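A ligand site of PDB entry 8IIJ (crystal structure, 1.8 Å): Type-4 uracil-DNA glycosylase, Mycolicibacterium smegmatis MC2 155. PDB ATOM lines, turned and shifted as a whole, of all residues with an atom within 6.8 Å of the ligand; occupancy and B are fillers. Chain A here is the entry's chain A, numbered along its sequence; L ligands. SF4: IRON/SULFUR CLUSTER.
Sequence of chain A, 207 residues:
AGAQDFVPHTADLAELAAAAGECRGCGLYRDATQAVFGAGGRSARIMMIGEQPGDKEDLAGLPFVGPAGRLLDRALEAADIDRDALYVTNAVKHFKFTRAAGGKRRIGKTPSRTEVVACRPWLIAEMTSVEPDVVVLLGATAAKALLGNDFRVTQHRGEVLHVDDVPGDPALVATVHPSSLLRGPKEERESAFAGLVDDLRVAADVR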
ATOM      1  N   GLY A   2     -29.237  33.781   5.806  1.00  0.00           N
ATOM      2  CA  GLY A   2     -28.535  32.545   5.487  1.00  0.00           C
ATOM      3  C   GLY A   2     -29.367  31.563   4.689  1.00  0.00           C
ATOM      4  O   GLY A   2     -30.001  31.903   3.685  1.00  0.00           O
ATOM      5  N   ALA A   3     -29.447  30.300   5.143  1.00  0.00           N
ATOM      6  CA  ALA A   3     -30.126  29.186   4.420  1.00  0.00           C
ATOM      7  C   ALA A   3     -31.641  29.070   4.655  1.00  0.00           C
ATOM      8  O   ALA A   3     -32.245  28.223   4.052  1.00  0.00           O
ATOM      9  CB  ALA A   3     -29.478  27.912   4.877  1.00  0.00           C
ATOM     10  N   PHE A   6     -33.900  28.655   1.883  1.00  0.00           N
ATOM     11  CA  PHE A   6     -33.633  27.448   1.105  1.00  0.00           C
ATOM     12  C   PHE A   6     -34.164  26.189   1.760  1.00  0.00           C
ATOM     13  O   PHE A   6     -34.181  25.122   1.122  1.00  0.00           O
ATOM     14  CB  PHE A   6     -32.139  27.328   0.872  1.00  0.00           C
ATOM     15  CG  PHE A   6     -31.600  28.424   0.026  1.00  0.00           C
ATOM     16  CD1 PHE A   6     -31.788  28.409  -1.348  1.00  0.00           C
ATOM     17  CD2 PHE A   6     -30.994  29.534   0.612  1.00  0.00           C
ATOM     18  CE1 PHE A   6     -31.332  29.440  -2.148  1.00  0.00           C
ATOM     19  CE2 PHE A   6     -30.517  30.589  -0.191  1.00  0.00           C
ATOM     20  CZ  PHE A   6     -30.682  30.541  -1.569  1.00  0.00           C
ATOM     21  N   ALA A  20     -30.830  20.954   0.343  1.00  0.00           N
ATOM     22  CA  ALA A  20     -29.493  21.436   0.695  1.00  0.00           C
ATOM     23  C   ALA A  20     -28.577  21.420  -0.508  1.00  0.00           C
ATOM     24  O   ALA A  20     -27.689  22.272  -0.610  1.00  0.00           O
ATOM     25  CB  ALA A  20     -28.906  20.568   1.821  1.00  0.00           C
ATOM     26  N   GLY A  21     -28.772  20.477  -1.432  1.00  0.00           N
ATOM     27  CA  GLY A  21     -27.983  20.498  -2.649  1.00  0.00           C
ATOM     28  C   GLY A  21     -28.137  21.783  -3.443  1.00  0.00           C
ATOM     29  O   GLY A  21     -27.256  22.128  -4.238  1.00  0.00           O
ATOM     30  N   GLU A  22     -29.250  22.504  -3.241  1.00  0.00           N
ATOM     31  CA  GLU A  22     -29.551  23.751  -3.939  1.00  0.00           C
ATOM     32  C   GLU A  22     -29.289  24.991  -3.093  1.00  0.00           C
ATOM     33  O   GLU A  22     -29.550  26.100  -3.568  1.00  0.00           O
ATOM     34  CB  GLU A  22     -31.024  23.761  -4.371  1.00  0.00           C
ATOM     35  CG  GLU A  22     -31.504  22.501  -5.035  1.00  0.00           C
ATOM     36  CD  GLU A  22     -31.219  22.485  -6.519  1.00  0.00           C
ATOM     37  OE1 GLU A  22     -30.119  22.916  -6.929  1.00  0.00           O
ATOM     38  N   CYS A  23     -28.775  24.831  -1.879  1.00  0.00           N
ATOM     39  CA  CYS A  23     -28.606  25.978  -0.980  1.00  0.00           C
ATOM     40  C   CYS A  23     -27.539  26.924  -1.518  1.00  0.00           C
ATOM     41  O   CYS A  23     -26.481  26.495  -2.013  1.00  0.00           O
ATOM     42  CB  CYS A  23     -28.196  25.498   0.421  1.00  0.00           C
ATOM     43  SG  CYS A  23     -28.244  26.790   1.671  1.00  0.00           S
ATOM     44  N   ARG A  24     -27.821  28.238  -1.394  1.00  0.00           N
ATOM     45  CA  ARG A  24     -26.856  29.308  -1.609  1.00  0.00           C
ATOM     46  C   ARG A  24     -26.790  30.223  -0.391  1.00  0.00           C
ATOM     47  O   ARG A  24     -26.473  31.415  -0.519  1.00  0.00           O
ATOM     48  CB  ARG A  24     -27.177  30.106  -2.883  1.00  0.00           C
ATOM     49  CG  ARG A  24     -27.422  29.238  -4.120  1.00  0.00           C
ATOM     50  CD  ARG A  24     -27.636  30.058  -5.396  1.00  0.00           C
ATOM     51  NE  ARG A  24     -28.653  31.095  -5.239  1.00  0.00           N
ATOM     52  CZ  ARG A  24     -29.966  30.875  -5.308  1.00  0.00           C
ATOM     53  NH1 ARG A  24     -30.452  29.671  -5.546  1.00  0.00           N
ATOM     54  NH2 ARG A  24     -30.796  31.895  -5.131  1.00  0.00           N
ATOM     55  N   GLY A  25     -27.086  29.677   0.788  1.00  0.00           N
ATOM     56  CA  GLY A  25     -27.182  30.471   2.009  1.00  0.00           C
ATOM     57  C   GLY A  25     -25.889  31.145   2.434  1.00  0.00           C
ATOM     58  O   GLY A  25     -25.951  32.109   3.198  1.00  0.00           O
ATOM     59  N   CYS A  26     -24.725  30.629   2.029  1.00  0.00           N
ATOM     60  CA  CYS A  26     -23.452  31.361   2.167  1.00  0.00           C
ATOM     61  C   CYS A  26     -22.619  31.081   0.928  1.00  0.00           C
ATOM     62  O   CYS A  26     -23.101  30.517  -0.063  1.00  0.00           O
ATOM     63  CB  CYS A  26     -22.708  30.991   3.450  1.00  0.00           C
ATOM     64  SG  CYS A  26     -21.989  29.305   3.450  1.00  0.00           S
ATOM     65  N   GLY A  27     -21.344  31.466   0.972  1.00  0.00           N
ATOM     66  CA  GLY A  27     -20.551  31.331  -0.242  1.00  0.00           C
ATOM     67  C   GLY A  27     -19.966  29.963  -0.477  1.00  0.00           C
ATOM     68  O   GLY A  27     -19.381  29.729  -1.545  1.00  0.00           O
ATOM     69  N   LEU A  28     -20.092  29.051   0.495  1.00  0.00           N
ATOM     70  CA  LEU A  28     -19.322  27.818   0.477  1.00  0.00           C
ATOM     71  C   LEU A  28     -19.793  26.833  -0.579  1.00  0.00           C
ATOM     72  O   LEU A  28     -19.018  25.965  -0.989  1.00  0.00           O
ATOM     73  CB  LEU A  28     -19.390  27.153   1.866  1.00  0.00           C
ATOM     74  CG  LEU A  28     -18.660  27.915   2.991  1.00  0.00           C
ATOM     75  CD1 LEU A  28     -18.753  27.150   4.333  1.00  0.00           C
ATOM     76  CD2 LEU A  28     -17.193  28.188   2.599  1.00  0.00           C
ATOM     77  N   TYR A  29     -21.060  26.922  -1.020  1.00  0.00           N
ATOM     78  CA  TYR A  29     -21.531  26.037  -2.078  1.00  0.00           C
ATOM     79  C   TYR A  29     -20.721  26.174  -3.374  1.00  0.00           C
ATOM     80  O   TYR A  29     -20.667  25.230  -4.158  1.00  0.00           O
ATOM     81  CB  TYR A  29     -23.025  26.292  -2.363  1.00  0.00           C
ATOM     82  CG  TYR A  29     -23.257  27.522  -3.234  1.00  0.00           C
ATOM     83  CD1 TYR A  29     -23.409  28.767  -2.648  1.00  0.00           C
ATOM     84  CD2 TYR A  29     -23.349  27.440  -4.626  1.00  0.00           C
ATOM     85  CE1 TYR A  29     -23.613  29.904  -3.403  1.00  0.00           C
ATOM     86  CE2 TYR A  29     -23.559  28.595  -5.410  1.00  0.00           C
ATOM     87  CZ  TYR A  29     -23.687  29.817  -4.788  1.00  0.00           C
ATOM     88  OH  TYR A  29     -23.904  30.976  -5.520  1.00  0.00           O
ATOM     89  N   ARG A  30     -20.106  27.337  -3.613  1.00  0.00           N
ATOM     90  CA  ARG A  30     -19.463  27.581  -4.935  1.00  0.00           C
ATOM     91  C   ARG A  30     -18.300  26.619  -5.213  1.00  0.00           C
ATOM     92  O   ARG A  30     -18.312  25.990  -6.268  1.00  0.00           O
ATOM     93  CB  ARG A  30     -19.034  29.038  -5.021  1.00  0.00           C
ATOM     94  CG  ARG A  30     -20.187  30.004  -5.190  1.00  0.00           C
ATOM     95  CD  ARG A  30     -19.754  31.401  -5.548  1.00  0.00           C
ATOM     96  NE  ARG A  30     -18.869  31.940  -4.523  1.00  0.00           N
ATOM     97  CZ  ARG A  30     -19.221  32.864  -3.643  1.00  0.00           C
ATOM     98  NH1 ARG A  30     -20.447  33.367  -3.654  1.00  0.00           N
ATOM     99  NH2 ARG A  30     -18.343  33.294  -2.755  1.00  0.00           N
ATOM    100  N   ALA A  35     -23.389  19.356  -1.433  1.00  0.00           N
ATOM    101  CA  ALA A  35     -23.723  19.466  -0.007  1.00  0.00           C
ATOM    102  C   ALA A  35     -23.558  18.089   0.616  1.00  0.00           C
ATOM    103  O   ALA A  35     -23.827  17.096  -0.058  1.00  0.00           O
ATOM    104  CB  ALA A  35     -25.103  20.008   0.191  1.00  0.00           C
ATOM    105  N   ALA A  91     -22.095  21.027  11.336  1.00  0.00           N
ATOM    106  CA  ALA A  91     -22.644  22.378  11.521  1.00  0.00           C
ATOM    107  C   ALA A  91     -22.740  23.125  10.192  1.00  0.00           C
ATOM    108  O   ALA A  91     -23.677  23.913   9.977  1.00  0.00           O
ATOM    109  CB  ALA A  91     -21.788  23.163  12.505  1.00  0.00           C
ATOM    110  N   VAL A  92     -21.787  22.916   9.296  1.00  0.00           N
ATOM    111  CA  VAL A  92     -21.942  23.447   7.942  1.00  0.00           C
ATOM    112  C   VAL A  92     -21.822  22.289   6.945  1.00  0.00           C
ATOM    113  O   VAL A  92     -21.168  21.279   7.222  1.00  0.00           O
ATOM    114  CB  VAL A  92     -20.950  24.592   7.630  1.00  0.00           C
ATOM    115  CG1 VAL A  92     -20.950  25.658   8.766  1.00  0.00           C
ATOM    116  CG2 VAL A  92     -19.584  24.083   7.406  1.00  0.00           C
ATOM    117  N   LYS A  93     -22.503  22.439   5.812  1.00  0.00           N
ATOM    118  CA  LYS A  93     -22.785  21.315   4.909  1.00  0.00           C
ATOM    119  C   LYS A  93     -21.995  21.395   3.618  1.00  0.00           C
ATOM    120  O   LYS A  93     -22.118  20.482   2.799  1.00  0.00           O
ATOM    121  CB  LYS A  93     -24.270  21.257   4.542  1.00  0.00           C
ATOM    122  CG  LYS A  93     -25.276  21.208   5.691  1.00  0.00           C
ATOM    123  CD  LYS A  93     -25.099  20.081   6.621  1.00  0.00           C
ATOM    124  CE  LYS A  93     -26.454  19.780   7.259  1.00  0.00           C
ATOM    125  NZ  LYS A  93     -26.410  20.210   8.721  1.00  0.00           N
ATOM    126  N   HIS A  94     -21.210  22.453   3.460  1.00  0.00           N
ATOM    127  CA  HIS A  94     -20.298  22.570   2.295  1.00  0.00           C
ATOM    128  C   HIS A  94     -18.840  22.680   2.778  1.00  0.00           C
ATOM    129  O   HIS A  94     -18.584  23.469   3.675  1.00  0.00           O
ATOM    130  CB  HIS A  94     -20.698  23.719   1.356  1.00  0.00           C
ATOM    131  CG  HIS A  94     -21.658  23.306   0.310  1.00  0.00           C
ATOM    132  ND1 HIS A  94     -22.925  23.748   0.299  1.00  0.00           N
ATOM    133  CD2 HIS A  94     -21.541  22.490  -0.744  1.00  0.00           C
ATOM    134  CE1 HIS A  94     -23.577  23.246  -0.724  1.00  0.00           C
ATOM    135  NE2 HIS A  94     -22.741  22.471  -1.370  1.00  0.00           N
ATOM    136  N   PHE A  95     -17.962  21.853   2.216  1.00  0.00           N
ATOM    137  CA  PHE A  95     -16.544  21.861   2.541  1.00  0.00           C
ATOM    138  C   PHE A  95     -15.907  23.207   2.220  1.00  0.00           C
ATOM    139  O   PHE A  95     -15.922  23.642   1.066  1.00  0.00           O
ATOM    140  CB  PHE A  95     -15.879  20.731   1.749  1.00  0.00           C
ATOM    141  CG  PHE A  95     -14.401  20.529   2.000  1.00  0.00           C
ATOM    142  CD1 PHE A  95     -13.847  20.688   3.263  1.00  0.00           C
ATOM    143  CD2 PHE A  95     -13.581  20.083   0.959  1.00  0.00           C
ATOM    144  CE1 PHE A  95     -12.479  20.457   3.486  1.00  0.00           C
ATOM    145  CE2 PHE A  95     -12.212  19.837   1.165  1.00  0.00           C
ATOM    146  CZ  PHE A  95     -11.671  20.022   2.427  1.00  0.00           C
ATOM    147  N   GLU A 115     -20.699  31.902   8.602  1.00  0.00           N
ATOM    148  CA  GLU A 115     -21.087  30.689   7.879  1.00  0.00           C
ATOM    149  C   GLU A 115     -21.815  29.712   8.798  1.00  0.00           C
ATOM    150  O   GLU A 115     -22.766  29.048   8.358  1.00  0.00           O
ATOM    151  CB  GLU A 115     -19.856  30.022   7.251  1.00  0.00           C
ATOM    152  CG  GLU A 115     -19.333  30.864   6.077  1.00  0.00           C
ATOM    153  CD  GLU A 115     -17.845  30.734   5.791  1.00  0.00           C
ATOM    154  OE1 GLU A 115     -17.076  30.193   6.617  1.00  0.00           O
ATOM    155  OE2 GLU A 115     -17.448  31.171   4.698  1.00  0.00           O
ATOM    156  N   VAL A 117     -23.729  30.471  11.393  1.00  0.00           N
ATOM    157  CA  VAL A 117     -25.088  30.965  11.614  1.00  0.00           C
ATOM    158  C   VAL A 117     -25.935  30.814  10.339  1.00  0.00           C
ATOM    159  O   VAL A 117     -27.130  30.523  10.402  1.00  0.00           O
ATOM    160  CB  VAL A 117     -25.031  32.431  12.097  1.00  0.00           C
ATOM    161  CG1 VAL A 117     -26.415  33.083  12.069  1.00  0.00           C
ATOM    162  CG2 VAL A 117     -24.406  32.516  13.492  1.00  0.00           C
ATOM    163  N   ALA A 118     -25.315  31.029   9.174  1.00  0.00           N
ATOM    164  CA  ALA A 118     -26.037  30.926   7.903  1.00  0.00           C
ATOM    165  C   ALA A 118     -26.545  29.508   7.660  1.00  0.00           C
ATOM    166  O   ALA A 118     -27.632  29.308   7.117  1.00  0.00           O
ATOM    167  CB  ALA A 118     -25.110  31.352   6.751  1.00  0.00           C
ATOM    168  N   CYS A 119     -25.754  28.504   8.056  1.00  0.00           N
ATOM    169  CA  CYS A 119     -26.108  27.110   7.810  1.00  0.00           C
ATOM    170  C   CYS A 119     -26.966  26.533   8.914  1.00  0.00           C
ATOM    171  O   CYS A 119     -27.625  25.519   8.706  1.00  0.00           O
ATOM    172  CB  CYS A 119     -24.839  26.250   7.665  1.00  0.00           C
ATOM    173  SG  CYS A 119     -25.049  24.806   6.622  1.00  0.00           S
ATOM    174  N   ARG A 120     -27.003  27.198  10.075  1.00  0.00           N
ATOM    175  CA  ARG A 120     -27.694  26.629  11.217  1.00  0.00           C
ATOM    176  C   ARG A 120     -29.162  26.275  10.939  1.00  0.00           C
ATOM    177  O   ARG A 120     -29.631  25.301  11.551  1.00  0.00           O
ATOM    178  CB  ARG A 120     -27.573  27.595  12.420  1.00  0.00           C
ATOM    179  CG  ARG A 120     -28.118  26.958  13.711  1.00  0.00           C
ATOM    180  CD  ARG A 120     -27.735  27.731  14.973  1.00  0.00           C
ATOM    181  NE  ARG A 120     -28.049  29.153  14.853  1.00  0.00           N
ATOM    182  CZ  ARG A 120     -27.428  30.120  15.516  1.00  0.00           C
ATOM    183  NH1 ARG A 120     -26.481  29.853  16.398  1.00  0.00           N
ATOM    184  NH2 ARG A 120     -27.767  31.382  15.295  1.00  0.00           N
ATOM    185  N   PRO A 121     -29.909  26.959  10.056  1.00  0.00           N
ATOM    186  CA  PRO A 121     -31.279  26.485   9.769  1.00  0.00           C
ATOM    187  C   PRO A 121     -31.364  25.026   9.310  1.00  0.00           C
ATOM    188  O   PRO A 121     -32.366  24.360   9.611  1.00  0.00           O
ATOM    189  CB  PRO A 121     -31.778  27.472   8.688  1.00  0.00           C
ATOM    190  CG  PRO A 121     -30.942  28.728   8.866  1.00  0.00           C
ATOM    191  CD  PRO A 121     -29.634  28.297   9.472  1.00  0.00           C
ATOM    192  N   TRP A 122     -30.361  24.505   8.582  1.00  0.00           N
ATOM    193  CA  TRP A 122     -30.359  23.069   8.267  1.00  0.00           C
ATOM    194  C   TRP A 122     -30.279  22.236   9.536  1.00  0.00           C
ATOM    195  O   TRP A 122     -31.004  21.250   9.683  1.00  0.00           O
ATOM    196  CB  TRP A 122     -29.179  22.736   7.342  1.00  0.00           C
ATOM    197  CG  TRP A 122     -29.344  23.352   5.999  1.00  0.00           C
ATOM    198  CD1 TRP A 122     -28.514  24.264   5.380  1.00  0.00           C
ATOM    199  CD2 TRP A 122     -30.394  23.059   5.062  1.00  0.00           C
ATOM    200  NE1 TRP A 122     -29.017  24.573   4.115  1.00  0.00           N
ATOM    201  CE2 TRP A 122     -30.162  23.849   3.909  1.00  0.00           C
ATOM    202  CE3 TRP A 122     -31.501  22.201   5.088  1.00  0.00           C
ATOM    203  CZ2 TRP A 122     -31.013  23.808   2.801  1.00  0.00           C
ATOM    204  CZ3 TRP A 122     -32.358  22.187   3.991  1.00  0.00           C
ATOM    205  CH2 TRP A 122     -32.106  22.963   2.860  1.00  0.00           C
HETATM  206 FE1  SF4 L   1     -24.700  25.584   4.565  1.00  0.00          FE
HETATM  207 FE2  SF4 L   1     -23.676  27.723   3.185  1.00  0.00          FE
HETATM  208 FE3  SF4 L   1     -26.092  26.597   2.396  1.00  0.00          FE
HETATM  209 FE4  SF4 L   1     -23.793  25.233   2.070  1.00  0.00          FE
HETATM  210  S1  SF4 L   1     -24.380  27.243   1.026  1.00  0.00           S
HETATM  211  S2  SF4 L   1     -25.729  24.360   2.885  1.00  0.00           S
HETATM  212  S3  SF4 L   1     -22.535  25.838   3.920  1.00  0.00           S
HETATM  213  S4  SF4 L   1     -25.615  27.691   4.375  1.00  0.00           S
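N of Cys 119 lies close to S4 of the ligand (3.8 Å).
The side-chain sulfur (SG) of Cys 119 binds an iron atom (FE1) of the ligand, 2.2 Å away.
SG of Cys 23 binds FE3 of the ligand, 2.3 Å away.
The backbone NH (N) of Cys 26 lies close to a sulfur (S1) of the ligand (3.5 Å).
An iron atom (FE2) of the ligand is bound by the side-chain sulfur (SG) of Cys 26, 2.3 Å away.
The backbone NH (N) of His 94 lies close to a sulfur (S3) of the ligand, 3.7 Å away.
A ring nitrogen (ND1) of His 94 is bound to an iron atom (FE4) of the ligand, 2.5 Å away.
S2 of the ligand lies close to NE1 of Trp 122 (3.5 Å).
N of Gly 25 sits close to S1 of the ligand (3.6 Å).
SG of Cys 119 lies close to N of Lys 93.
The backbone carbonyl oxygen of Ala 91 sits close to the side-chain sulfur of Cys 119.
NE1 of Trp 122 sits close to SG of Cys 23, at 3.4 Å.
The backbone NH (N) of Gly 25 lies close to the side-chain sulfur (SG) of Cys 23 (3.2 Å).
The side-chain sulfur (SG) of Cys 26 sits close to the backbone NH (N) of Leu 28 (3.5 Å).
A ring nitrogen (NE2) of His 94 sits at hydrogen-bond distance from the backbone NH (N) of Ala 35, at 3.2 Å.
The backbone carbonyl oxygen of Ala 118 sits at hydrogen-bond distance from the backbone NH of Ala 3, 2.9 Å away.
O of Ala 118 lies close to S4 of the ligand (3.8 Å).
Residues that only touch the ligand: Tyr 29, Lys 93, Ala 3 and Leu 28.
Hydrophobic or aromatic side chains within 4 Å of the ligand: Ala 3, Leu 28, Tyr 29, His 94 and Trp 122.
11 residues have an atom within 4 Å of the ligand: Ala 3, Cys 23, Gly 25, Cys 26, Leu 28, Tyr 29, Lys 93, His 94, Ala 118, Cys 119 and Trp 122.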
